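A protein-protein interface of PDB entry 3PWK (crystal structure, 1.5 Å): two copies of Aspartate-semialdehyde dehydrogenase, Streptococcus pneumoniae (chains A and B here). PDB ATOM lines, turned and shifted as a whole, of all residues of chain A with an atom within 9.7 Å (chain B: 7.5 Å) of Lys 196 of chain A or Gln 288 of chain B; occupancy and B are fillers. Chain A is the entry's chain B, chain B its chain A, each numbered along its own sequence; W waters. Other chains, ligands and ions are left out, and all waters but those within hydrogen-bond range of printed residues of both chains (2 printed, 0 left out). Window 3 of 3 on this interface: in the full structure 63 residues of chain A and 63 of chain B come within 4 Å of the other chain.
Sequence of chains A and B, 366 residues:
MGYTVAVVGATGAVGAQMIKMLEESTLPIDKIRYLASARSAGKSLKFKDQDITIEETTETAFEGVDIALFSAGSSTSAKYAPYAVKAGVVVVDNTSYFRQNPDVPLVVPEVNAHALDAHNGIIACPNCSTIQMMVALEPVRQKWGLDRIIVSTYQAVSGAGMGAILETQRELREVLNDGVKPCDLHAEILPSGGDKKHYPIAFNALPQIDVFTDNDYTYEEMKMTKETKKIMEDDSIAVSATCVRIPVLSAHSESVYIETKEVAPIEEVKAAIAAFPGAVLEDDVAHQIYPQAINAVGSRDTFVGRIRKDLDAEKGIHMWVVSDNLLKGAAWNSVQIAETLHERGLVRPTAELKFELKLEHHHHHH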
ATOM      1  N   ALA A 187      -1.835  -5.030  -7.033  1.00  0.00           N
ATOM      2  CA  ALA A 187      -2.563  -4.433  -8.153  1.00  0.00           C
ATOM      3  C   ALA A 187      -2.524  -2.907  -8.081  1.00  0.00           C
ATOM      4  O   ALA A 187      -2.478  -2.332  -6.979  1.00  0.00           O
ATOM      5  CB  ALA A 187      -4.009  -4.929  -8.167  1.00  0.00           C
ATOM      6  N   GLU A 188      -2.544  -2.268  -9.251  1.00  0.00           N
ATOM      7  CA  GLU A 188      -2.486  -0.805  -9.367  1.00  0.00           C
ATOM      8  C   GLU A 188      -3.686  -0.184 -10.078  1.00  0.00           C
ATOM      9  O   GLU A 188      -3.960   1.002  -9.897  1.00  0.00           O
ATOM     10  CB  GLU A 188      -1.188  -0.356 -10.058  1.00  0.00           C
ATOM     11  CG  GLU A 188       0.074  -0.970  -9.440  1.00  0.00           C
ATOM     12  CD  GLU A 188       1.335  -0.185  -9.734  1.00  0.00           C
ATOM     13  OE1 GLU A 188       1.650   0.019 -10.925  1.00  0.00           O
ATOM     14  OE2 GLU A 188       2.030   0.204  -8.769  1.00  0.00           O
ATOM     15  N   ILE A 189      -4.393  -0.976 -10.889  1.00  0.00           N
ATOM     16  CA  ILE A 189      -5.439  -0.429 -11.766  1.00  0.00           C
ATOM     17  C   ILE A 189      -6.801  -1.038 -11.435  1.00  0.00           C
ATOM     18  O   ILE A 189      -7.723  -0.323 -11.018  1.00  0.00           O
ATOM     19  CB  ILE A 189      -5.095  -0.641 -13.251  1.00  0.00           C
ATOM     20  CG1 ILE A 189      -3.799   0.121 -13.596  1.00  0.00           C
ATOM     21  CG2 ILE A 189      -6.245  -0.153 -14.135  1.00  0.00           C
ATOM     22  CD1 ILE A 189      -3.183  -0.275 -14.904  1.00  0.00           C
ATOM     23  N   LEU A 190      -6.945  -2.353 -11.609  1.00  0.00           N
ATOM     24  CA  LEU A 190      -8.267  -2.984 -11.401  1.00  0.00           C
ATOM     25  C   LEU A 190      -8.640  -3.010  -9.913  1.00  0.00           C
ATOM     26  O   LEU A 190      -7.758  -3.016  -9.063  1.00  0.00           O
ATOM     27  CB  LEU A 190      -8.289  -4.388 -11.997  1.00  0.00           C
ATOM     28  CG  LEU A 190      -8.149  -4.394 -13.524  1.00  0.00           C
ATOM     29  CD1 LEU A 190      -7.742  -5.781 -13.988  1.00  0.00           C
ATOM     30  CD2 LEU A 190      -9.408  -3.872 -14.272  1.00  0.00           C
ATOM     31  N   PRO A 191      -9.946  -3.015  -9.597  1.00  0.00           N
ATOM     32  CA  PRO A 191     -11.080  -3.026 -10.530  1.00  0.00           C
ATOM     33  C   PRO A 191     -11.329  -1.720 -11.287  1.00  0.00           C
ATOM     34  O   PRO A 191     -11.863  -1.763 -12.406  1.00  0.00           O
ATOM     35  CB  PRO A 191     -12.272  -3.373  -9.634  1.00  0.00           C
ATOM     36  CG  PRO A 191     -11.869  -2.866  -8.249  1.00  0.00           C
ATOM     37  CD  PRO A 191     -10.378  -3.104  -8.189  1.00  0.00           C
ATOM     38  N   SER A 192     -10.958  -0.577 -10.703  1.00  0.00           N
ATOM     39  CA  SER A 192     -11.250   0.719 -11.320  1.00  0.00           C
ATOM     40  C   SER A 192     -10.092   1.682 -11.080  1.00  0.00           C
ATOM     41  O   SER A 192      -9.781   2.011  -9.933  1.00  0.00           O
ATOM     42  CB  SER A 192     -12.549   1.299 -10.758  1.00  0.00           C
ATOM     43  OG  SER A 192     -12.746   2.623 -11.219  1.00  0.00           O
ATOM     44  N   GLY A 193      -9.470   2.126 -12.165  1.00  0.00           N
ATOM     45  CA  GLY A 193      -8.263   2.935 -12.087  1.00  0.00           C
ATOM     46  C   GLY A 193      -8.413   4.133 -11.180  1.00  0.00           C
ATOM     47  O   GLY A 193      -7.499   4.442 -10.400  1.00  0.00           O
ATOM     48  N   GLY A 194      -9.568   4.791 -11.250  1.00  0.00           N
ATOM     49  CA  GLY A 194      -9.786   6.021 -10.474  1.00  0.00           C
ATOM     50  C   GLY A 194     -10.176   5.845  -9.013  1.00  0.00           C
ATOM     51  O   GLY A 194     -10.099   6.798  -8.222  1.00  0.00           O
ATOM     52  N   ASP A 195     -10.587   4.633  -8.639  1.00  0.00           N
ATOM     53  CA  ASP A 195     -11.065   4.392  -7.285  1.00  0.00           C
ATOM     54  C   ASP A 195      -9.906   4.237  -6.293  1.00  0.00           C
ATOM     55  O   ASP A 195      -8.739   4.214  -6.688  1.00  0.00           O
ATOM     56  CB  ASP A 195     -12.010   3.179  -7.256  1.00  0.00           C
ATOM     57  CG  ASP A 195     -13.157   3.343  -6.258  1.00  0.00           C
ATOM     58  OD1 ASP A 195     -13.057   4.207  -5.351  1.00  0.00           O
ATOM     59  OD2 ASP A 195     -14.156   2.592  -6.365  1.00  0.00           O
ATOM     60  N   LYS A 196     -10.238   4.122  -5.013  1.00  0.00           N
ATOM     61  CA  LYS A 196      -9.251   4.242  -3.937  1.00  0.00           C
ATOM     62  C   LYS A 196      -8.395   3.000  -3.710  1.00  0.00           C
ATOM     63  O   LYS A 196      -7.222   3.108  -3.319  1.00  0.00           O
ATOM     64  CB  LYS A 196      -9.952   4.609  -2.629  1.00  0.00           C
ATOM     65  CG  LYS A 196     -10.698   5.938  -2.669  1.00  0.00           C
ATOM     66  CD  LYS A 196     -11.388   6.188  -1.343  1.00  0.00           C
ATOM     67  CE  LYS A 196     -12.399   7.315  -1.436  1.00  0.00           C
ATOM     68  NZ  LYS A 196     -11.774   8.615  -1.820  1.00  0.00           N
ATOM     69  N   LYS A 197      -8.978   1.829  -3.932  1.00  0.00           N
ATOM     70  CA  LYS A 197      -8.304   0.564  -3.659  1.00  0.00           C
ATOM     71  C   LYS A 197      -8.266  -0.308  -4.897  1.00  0.00           C
ATOM     72  O   LYS A 197      -9.198  -0.289  -5.703  1.00  0.00           O
ATOM     73  CB  LYS A 197      -9.023  -0.177  -2.533  1.00  0.00           C
ATOM     74  CG  LYS A 197      -9.061   0.627  -1.231  1.00  0.00           C
ATOM     75  CD  LYS A 197     -10.134   0.108  -0.293  1.00  0.00           C
ATOM     76  CE  LYS A 197      -9.763  -1.235   0.294  1.00  0.00           C
ATOM     77  NZ  LYS A 197     -10.791  -1.692   1.271  1.00  0.00           N
ATOM     78  N   HIS A 198      -7.178  -1.057  -5.039  1.00  0.00           N
ATOM     79  CA  HIS A 198      -6.982  -1.955  -6.173  1.00  0.00           C
ATOM     80  C   HIS A 198      -6.798  -3.398  -5.727  1.00  0.00           C
ATOM     81  O   HIS A 198      -6.170  -3.666  -4.693  1.00  0.00           O
ATOM     82  CB  HIS A 198      -5.809  -1.448  -7.006  1.00  0.00           C
ATOM     83  CG  HIS A 198      -5.936   0.005  -7.341  1.00  0.00           C
ATOM     84  ND1 HIS A 198      -6.809   0.473  -8.304  1.00  0.00           N
ATOM     85  CD2 HIS A 198      -5.369   1.100  -6.780  1.00  0.00           C
ATOM     86  CE1 HIS A 198      -6.750   1.792  -8.340  1.00  0.00           C
ATOM     87  NE2 HIS A 198      -5.880   2.197  -7.431  1.00  0.00           N
ATOM     88  N   TYR A 199      -7.330  -4.319  -6.521  1.00  0.00           N
ATOM     89  CA  TYR A 199      -7.346  -5.746  -6.188  1.00  0.00           C
ATOM     90  C   TYR A 199      -6.851  -6.595  -7.355  1.00  0.00           C
ATOM     91  O   TYR A 199      -7.059  -6.221  -8.524  1.00  0.00           O
ATOM     92  CB  TYR A 199      -8.772  -6.183  -5.851  1.00  0.00           C
ATOM     93  CG  TYR A 199      -9.434  -5.423  -4.715  1.00  0.00           C
ATOM     94  CD1 TYR A 199      -8.824  -5.323  -3.449  1.00  0.00           C
ATOM     95  CD2 TYR A 199     -10.696  -4.847  -4.890  1.00  0.00           C
ATOM     96  CE1 TYR A 199      -9.439  -4.645  -2.407  1.00  0.00           C
ATOM     97  CE2 TYR A 199     -11.325  -4.167  -3.847  1.00  0.00           C
ATOM     98  CZ  TYR A 199     -10.692  -4.065  -2.612  1.00  0.00           C
ATOM     99  OH  TYR A 199     -11.311  -3.407  -1.573  1.00  0.00           O
ATOM    100  N   LEU A 206     -14.142  -9.996  -9.903  1.00  0.00           N
ATOM    101  CA  LEU A 206     -14.327  -8.746  -9.131  1.00  0.00           C
ATOM    102  C   LEU A 206     -15.688  -8.144  -9.500  1.00  0.00           C
ATOM    103  O   LEU A 206     -15.861  -7.676 -10.625  1.00  0.00           O
ATOM    104  CB  LEU A 206     -13.221  -7.739  -9.469  1.00  0.00           C
ATOM    105  CG  LEU A 206     -11.816  -8.048  -8.948  1.00  0.00           C
ATOM    106  CD1 LEU A 206     -10.801  -7.115  -9.572  1.00  0.00           C
ATOM    107  CD2 LEU A 206     -11.796  -7.950  -7.416  1.00  0.00           C
ATOM    108  N   PRO A 207     -16.651  -8.140  -8.557  1.00  0.00           N
ATOM    109  CA  PRO A 207     -18.005  -7.590  -8.839  1.00  0.00           C
ATOM    110  C   PRO A 207     -18.024  -6.053  -8.715  1.00  0.00           C
ATOM    111  O   PRO A 207     -18.842  -5.472  -7.981  1.00  0.00           O
ATOM    112  CB  PRO A 207     -18.862  -8.249  -7.759  1.00  0.00           C
ATOM    113  CG  PRO A 207     -17.908  -8.327  -6.588  1.00  0.00           C
ATOM    114  CD  PRO A 207     -16.547  -8.656  -7.177  1.00  0.00           C
ATOM    115  N   GLN A 208     -17.076  -5.407  -9.383  1.00  0.00           N
ATOM    116  CA  GLN A 208     -17.028  -3.945  -9.452  1.00  0.00           C
ATOM    117  C   GLN A 208     -16.409  -3.558 -10.785  1.00  0.00           C
ATOM    118  O   GLN A 208     -15.250  -3.922 -11.074  1.00  0.00           O
ATOM    119  CB  GLN A 208     -16.187  -3.325  -8.318  1.00  0.00           C
ATOM    120  CG  GLN A 208     -16.214  -1.797  -8.428  1.00  0.00           C
ATOM    121  CD  GLN A 208     -15.242  -1.048  -7.511  1.00  0.00           C
ATOM    122  OE1 GLN A 208     -14.689  -1.593  -6.548  1.00  0.00           O
ATOM    123  NE2 GLN A 208     -15.064   0.235  -7.801  1.00  0.00           N
ATOM    124  N   ILE A 209     -17.200  -2.855 -11.591  1.00  0.00           N
ATOM    125  CA  ILE A 209     -16.706  -2.165 -12.781  1.00  0.00           C
ATOM    126  C   ILE A 209     -17.143  -0.707 -12.673  1.00  0.00           C
ATOM    127  O   ILE A 209     -18.301  -0.417 -12.357  1.00  0.00           O
ATOM    128  CB  ILE A 209     -17.176  -2.868 -14.085  1.00  0.00           C
ATOM    129  CG1 ILE A 209     -16.571  -4.287 -14.114  1.00  0.00           C
ATOM    130  CG2 ILE A 209     -16.773  -2.075 -15.316  1.00  0.00           C
ATOM    131  CD1 ILE A 209     -16.930  -5.128 -15.297  1.00  0.00           C
ATOM    132  N   ASP A 210     -16.197   0.204 -12.901  1.00  0.00           N
ATOM    133  CA  ASP A 210     -16.371   1.636 -12.587  1.00  0.00           C
ATOM    134  C   ASP A 210     -16.542   1.835 -11.077  1.00  0.00           C
ATOM    135  O   ASP A 210     -16.319   0.909 -10.286  1.00  0.00           O
ATOM    136  CB  ASP A 210     -17.573   2.227 -13.361  1.00  0.00           C
ATOM    137  CG  ASP A 210     -17.341   3.654 -13.835  1.00  0.00           C
ATOM    138  OD1 ASP A 210     -16.960   4.526 -13.030  1.00  0.00           O
ATOM    139  OD2 ASP A 210     -17.594   3.906 -15.039  1.00  0.00           O
ATOM    140  N   VAL A 211     -16.935   3.036 -10.673  1.00  0.00           N
ATOM    141  CA  VAL A 211     -17.072   3.346  -9.249  1.00  0.00           C
ATOM    142  C   VAL A 211     -18.523   3.169  -8.804  1.00  0.00           C
ATOM    143  O   VAL A 211     -19.432   3.047  -9.642  1.00  0.00           O
ATOM    144  CB  VAL A 211     -16.544   4.769  -8.914  1.00  0.00           C
ATOM    145  CG1 VAL A 211     -15.075   4.873  -9.290  1.00  0.00           C
ATOM    146  CG2 VAL A 211     -17.354   5.818  -9.627  1.00  0.00           C
ATOM    147  N   PHE A 212     -18.744   3.137  -7.494  1.00  0.00           N
ATOM    148  CA  PHE A 212     -20.103   3.001  -6.979  1.00  0.00           C
ATOM    149  C   PHE A 212     -20.869   4.307  -7.071  1.00  0.00           C
ATOM    150  O   PHE A 212     -20.316   5.397  -6.845  1.00  0.00           O
ATOM    151  CB  PHE A 212     -20.085   2.471  -5.539  1.00  0.00           C
ATOM    152  CG  PHE A 212     -19.768   1.014  -5.467  1.00  0.00           C
ATOM    153  CD1 PHE A 212     -20.787   0.083  -5.633  1.00  0.00           C
ATOM    154  CD2 PHE A 212     -18.450   0.561  -5.294  1.00  0.00           C
ATOM    155  CE1 PHE A 212     -20.524  -1.299  -5.611  1.00  0.00           C
ATOM    156  CE2 PHE A 212     -18.166  -0.817  -5.277  1.00  0.00           C
ATOM    157  CZ  PHE A 212     -19.209  -1.753  -5.431  1.00  0.00           C
ATOM    158  N   THR A 218     -22.982   0.014  -9.352  1.00  0.00           N
ATOM    159  CA  THR A 218     -21.841   0.754  -9.907  1.00  0.00           C
ATOM    160  C   THR A 218     -22.279   1.548 -11.125  1.00  0.00           C
ATOM    161  O   THR A 218     -23.373   1.318 -11.678  1.00  0.00           O
ATOM    162  CB  THR A 218     -20.705  -0.177 -10.363  1.00  0.00           C
ATOM    163  OG1 THR A 218     -21.172  -0.974 -11.452  1.00  0.00           O
ATOM    164  CG2 THR A 218     -20.205  -1.069  -9.214  1.00  0.00           C
ATOM    165  N   GLU B 282     -19.770  -9.371   3.895  1.00  0.00           N
ATOM    166  CA  GLU B 282     -18.657  -8.537   3.431  1.00  0.00           C
ATOM    167  C   GLU B 282     -19.267  -7.554   2.463  1.00  0.00           C
ATOM    168  O   GLU B 282     -19.368  -7.822   1.262  1.00  0.00           O
ATOM    169  CB  GLU B 282     -17.556  -9.353   2.743  1.00  0.00           C
ATOM    170  CG  GLU B 282     -16.745 -10.192   3.666  1.00  0.00           C
ATOM    171  CD  GLU B 282     -15.610 -10.903   2.963  1.00  0.00           C
ATOM    172  OE1 GLU B 282     -15.730 -11.211   1.749  1.00  0.00           O
ATOM    173  OE2 GLU B 282     -14.609 -11.201   3.642  1.00  0.00           O
ATOM    174  N   ASP B 283     -19.732  -6.426   2.991  1.00  0.00           N
ATOM    175  CA  ASP B 283     -20.543  -5.524   2.189  1.00  0.00           C
ATOM    176  C   ASP B 283     -20.377  -4.118   2.734  1.00  0.00           C
ATOM    177  O   ASP B 283     -21.024  -3.729   3.711  1.00  0.00           O
ATOM    178  CB  ASP B 283     -22.009  -5.971   2.244  1.00  0.00           C
ATOM    179  CG  ASP B 283     -22.853  -5.413   1.106  1.00  0.00           C
ATOM    180  OD1 ASP B 283     -22.481  -4.365   0.537  1.00  0.00           O
ATOM    181  OD2 ASP B 283     -23.889  -6.035   0.788  1.00  0.00           O
ATOM    182  N   ASP B 284     -19.465  -3.379   2.124  1.00  0.00           N
ATOM    183  CA  ASP B 284     -19.192  -1.992   2.517  1.00  0.00           C
ATOM    184  C   ASP B 284     -18.670  -1.320   1.247  1.00  0.00           C
ATOM    185  O   ASP B 284     -17.460  -1.192   1.034  1.00  0.00           O
ATOM    186  CB  ASP B 284     -18.169  -1.934   3.667  1.00  0.00           C
ATOM    187  CG  ASP B 284     -17.824  -0.502   4.076  1.00  0.00           C
ATOM    188  OD1 ASP B 284     -18.443   0.461   3.556  1.00  0.00           O
ATOM    189  OD2 ASP B 284     -16.923  -0.350   4.914  1.00  0.00           O
ATOM    190  N   VAL B 285     -19.598  -0.924   0.387  1.00  0.00           N
ATOM    191  CA  VAL B 285     -19.204  -0.441  -0.937  1.00  0.00           C
ATOM    192  C   VAL B 285     -18.448   0.880  -0.874  1.00  0.00           C
ATOM    193  O   VAL B 285     -17.647   1.164  -1.757  1.00  0.00           O
ATOM    194  CB  VAL B 285     -20.389  -0.389  -1.945  1.00  0.00           C
ATOM    195  CG1 VAL B 285     -20.972  -1.787  -2.138  1.00  0.00           C
ATOM    196  CG2 VAL B 285     -21.452   0.590  -1.473  1.00  0.00           C
ATOM    197  N   ALA B 286     -18.665   1.663   0.193  1.00  0.00           N
ATOM    198  CA  ALA B 286     -17.917   2.909   0.381  1.00  0.00           C
ATOM    199  C   ALA B 286     -16.408   2.626   0.458  1.00  0.00           C
ATOM    200  O   ALA B 286     -15.598   3.499   0.145  1.00  0.00           O
ATOM    201  CB  ALA B 286     -18.383   3.642   1.648  1.00  0.00           C
ATOM    202  N   HIS B 287     -16.042   1.409   0.878  1.00  0.00           N
ATOM    203  CA  HIS B 287     -14.638   1.000   0.932  1.00  0.00           C
ATOM    204  C   HIS B 287     -14.338  -0.163  -0.007  1.00  0.00           C
ATOM    205  O   HIS B 287     -13.367  -0.896   0.185  1.00  0.00           O
ATOM    206  CB  HIS B 287     -14.216   0.673   2.381  1.00  0.00           C
ATOM    207  CG  HIS B 287     -14.385   1.826   3.318  1.00  0.00           C
ATOM    208  ND1 HIS B 287     -15.372   1.864   4.276  1.00  0.00           N
ATOM    209  CD2 HIS B 287     -13.721   3.003   3.414  1.00  0.00           C
ATOM    210  CE1 HIS B 287     -15.285   3.001   4.950  1.00  0.00           C
ATOM    211  NE2 HIS B 287     -14.297   3.715   4.438  1.00  0.00           N
ATOM    212  N   GLN B 288     -15.179  -0.306  -1.037  1.00  0.00           N
ATOM    213  CA  GLN B 288     -15.000  -1.346  -2.042  1.00  0.00           C
ATOM    214  C   GLN B 288     -14.840  -2.738  -1.424  1.00  0.00           C
ATOM    215  O   GLN B 288     -14.003  -3.553  -1.869  1.00  0.00           O
ATOM    216  CB  GLN B 288     -13.806  -1.045  -2.936  1.00  0.00           C
ATOM    217  CG  GLN B 288     -13.900   0.237  -3.750  1.00  0.00           C
ATOM    218  CD  GLN B 288     -12.575   0.539  -4.409  1.00  0.00           C
ATOM    219  OE1 GLN B 288     -11.790   1.351  -3.905  1.00  0.00           O
ATOM    220  NE2 GLN B 288     -12.291  -0.149  -5.508  1.00  0.00           N
ATOM    221  N   ILE B 289     -15.654  -3.018  -0.414  1.00  0.00           N
ATOM    222  CA  ILE B 289     -15.647  -4.326   0.234  1.00  0.00           C
ATOM    223  C   ILE B 289     -16.798  -5.169  -0.298  1.00  0.00           C
ATOM    224  O   ILE B 289     -17.968  -4.785  -0.215  1.00  0.00           O
ATOM    225  CB  ILE B 289     -15.768  -4.200   1.766  1.00  0.00           C
ATOM    226  CG1 ILE B 289     -14.621  -3.361   2.337  1.00  0.00           C
ATOM    227  CG2 ILE B 289     -15.845  -5.586   2.428  1.00  0.00           C
ATOM    228  CD1 ILE B 289     -13.246  -3.871   2.041  1.00  0.00           C
ATOM    229  N   TYR B 290     -16.440  -6.321  -0.858  1.00  0.00           N
ATOM    230  CA  TYR B 290     -17.413  -7.313  -1.357  1.00  0.00           C
ATOM    231  C   TYR B 290     -16.683  -8.658  -1.377  1.00  0.00           C
ATOM    232  O   TYR B 290     -15.450  -8.692  -1.371  1.00  0.00           O
ATOM    233  CB  TYR B 290     -17.914  -6.965  -2.786  1.00  0.00           C
ATOM    234  CG  TYR B 290     -16.884  -6.219  -3.617  1.00  0.00           C
ATOM    235  CD1 TYR B 290     -15.739  -6.874  -4.122  1.00  0.00           C
ATOM    236  CD2 TYR B 290     -17.039  -4.844  -3.871  1.00  0.00           C
ATOM    237  CE1 TYR B 290     -14.788  -6.174  -4.883  1.00  0.00           C
ATOM    238  CE2 TYR B 290     -16.097  -4.132  -4.616  1.00  0.00           C
ATOM    239  CZ  TYR B 290     -14.972  -4.806  -5.126  1.00  0.00           C
ATOM    240  OH  TYR B 290     -14.034  -4.120  -5.866  1.00  0.00           O
ATOM    241  N   PRO B 291     -17.427  -9.774  -1.402  1.00  0.00           N
ATOM    242  CA  PRO B 291     -16.771 -11.085  -1.493  1.00  0.00           C
ATOM    243  C   PRO B 291     -15.881 -11.226  -2.728  1.00  0.00           C
ATOM    244  O   PRO B 291     -16.220 -10.718  -3.801  1.00  0.00           O
ATOM    245  CB  PRO B 291     -17.957 -12.065  -1.558  1.00  0.00           C
ATOM    246  CG  PRO B 291     -19.068 -11.317  -0.835  1.00  0.00           C
ATOM    247  CD  PRO B 291     -18.888  -9.895  -1.297  1.00  0.00           C
ATOM    248  N   GLN B 292     -14.746 -11.896  -2.553  1.00  0.00           N
ATOM    249  CA  GLN B 292     -13.825 -12.179  -3.667  1.00  0.00           C
ATOM    250  C   GLN B 292     -13.315 -13.604  -3.584  1.00  0.00           C
ATOM    251  O   GLN B 292     -12.856 -14.034  -2.523  1.00  0.00           O
ATOM    252  CB  GLN B 292     -12.612 -11.243  -3.658  1.00  0.00           C
ATOM    253  CG  GLN B 292     -12.941  -9.774  -3.835  1.00  0.00           C
ATOM    254  CD  GLN B 292     -11.681  -8.931  -3.898  1.00  0.00           C
ATOM    255  OE1 GLN B 292     -10.687  -9.339  -4.499  1.00  0.00           O
ATOM    256  NE2 GLN B 292     -11.724  -7.736  -3.306  1.00  0.00           N
HETATM  257  O   HOH W   1     -14.239   4.279  -2.855  1.00  0.00           O
HETATM  258  O   HOH W   2     -10.120   0.109  -8.084  1.00  0.00           O
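Lys 196 of chain A touches one residue of chain B. Of chain A, only Pro 191, Asp 195, Lys 196, Lys 197, Tyr 199 and Gln 208 come within 4 Å of Gln 288 of chain B. Of chain A, only Lys 197 (3.4 Å) comes within 4 Å of Ile 289 of chain B. Printed residues of chain B within 4 Å of Tyr 199 of chain A: His 287 (3.7 Å), Gln 288 (2.7 Å), Tyr 290 (3.4 Å) and Gln 292 (3.5 Å). Printed residues of chain B within 4 Å of Phe 212 of chain A: Val 285 (3.5 Å) and Tyr 290 (3.96 Å). Printed residues of chain A within 4 Å of His 287 of chain B: Lys 197 and Tyr 199. Printed residues of chain B within 4 Å of Pro 191 of chain A: Gln 288 (3.9 Å) and Tyr 290 (3.5 Å). Of the printed residues of chain B, Leu 206 of chain A touches Gln 292 (3.4 Å). The nearest residue of chain B that does not touch Lys 196 of chain A is Ala 286 of chain B (5.2 Å). The nearest residue of chain A that does not touch Gln 288 of chain B is Phe 212 of chain A (4.6 Å). The nearest printed residue of chain B that does not touch Pro 191 of chain A is Gln 292 of chain B (6.9 Å).
The side-chain carboxylate (OD2) of Asp 284 of chain B is in hydrogen-bond range of a ring nitrogen (ND1) of His 287 of chain B (2.8 Å). The backbone carbonyl oxygen of Asp 284 of chain B is in hydrogen-bond range of the backbone NH of Ile 289 of chain B (2.9 Å). O of Leu 190 of chain A lies within hydrogen-bond range of N of Tyr 199 of chain A, 2.9 Å away. OD2 of Asp 195 of chain A sits at hydrogen-bond distance from NE2 of Gln 208 of chain A, 2.9 Å away. The side-chain amino group (NZ) of Lys 197 of chain A lies close to the side-chain hydroxyl (OH) of Tyr 199 of chain A, 3.4 Å away. The backbone carbonyl oxygen (O) of Asp 210 of chain A is in hydrogen-bond range of the side-chain amide nitrogen (NE2) of Gln 208 of chain A (2.9 Å).
Water W2 lies within hydrogen-bond range of O of Lys 197 of chain A (2.6 Å), O of Ser 192 of chain A (2.7 Å), ND1 of His 198 of chain A (3.3 Å) and NE2 of Gln 288 of chain B (3.4 Å). Water W1 lies within hydrogen-bond range of the side-chain carboxylate of Asp 195 of chain A and the backbone carbonyl oxygen of Ala 286 of chain B.
The backbone carbonyl oxygen (O) of His 287 of chain B lies within hydrogen-bond range of the side-chain amino group (NZ) of Lys 197 of chain A, 2.9 Å away. The side-chain amide nitrogen of Gln 288 of chain B sits close to the side-chain carboxylate of Asp 195 of chain A. The backbone NH (N) of Lys 196 of chain A sits at hydrogen-bond distance from the side-chain amide oxygen (OE1) of Gln 288 of chain B, at 3.4 Å. The backbone NH (N) of Lys 197 of chain A lies within hydrogen-bond range of the side-chain amide oxygen (OE1) of Gln 288 of chain B, at 2.9 Å. OH of Tyr 199 of chain A lies within hydrogen-bond range of O of Gln 288 of chain B, 2.7 Å away. The side-chain amide nitrogen (NE2) of Gln 288 of chain B lies within hydrogen-bond range of the side-chain amide oxygen (OE1) of Gln 208 of chain A (3.0 Å). The side-chain hydroxyl (OH) of Tyr 290 of chain B is in hydrogen-bond range of the side-chain amide oxygen (OE1) of Gln 208 of chain A, 2.7 Å away.
No position is printed for both chains. Of the 18 pairs that touch across the chains among the printed residues, none has its exchanged pair printed and touching as well.
Among the printed residues, merely in contact across the chains: Lys 197 of chain A with Ile 289 of chain B (3.4 Å), Tyr 199 of chain A with Tyr 290 of chain B (3.4 Å), Leu 206 of chain A with Gln 292 of chain B (3.4 Å), Tyr 199 of chain A with Gln 292 of chain B (3.5 Å), Pro 191 of chain A with Tyr 290 of chain B (3.5 Å), Phe 212 of chain A with Val 285 of chain B (3.5 Å), Pro 207 of chain A with Tyr 290 of chain B (3.6 Å), Tyr 199 of chain A with His 287 of chain B (3.7 Å), Pro 191 of chain A with Gln 288 of chain B (3.9 Å), Phe 212 of chain A with Tyr 290 of chain B (3.96 Å) and Pro 207 of chain A with Pro 291 of chain B (3.97 Å).
Of the 11 printed residues of chain B, 7 touch a printed residue of chain A. Of the 21 printed residues of chain A, 9 touch a printed residue of chain B. Hydrophobic or aromatic side chains of chain A that line the printed part of chain B: Pro 191, Tyr 199, Leu 206, Pro 207 and Phe 212.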
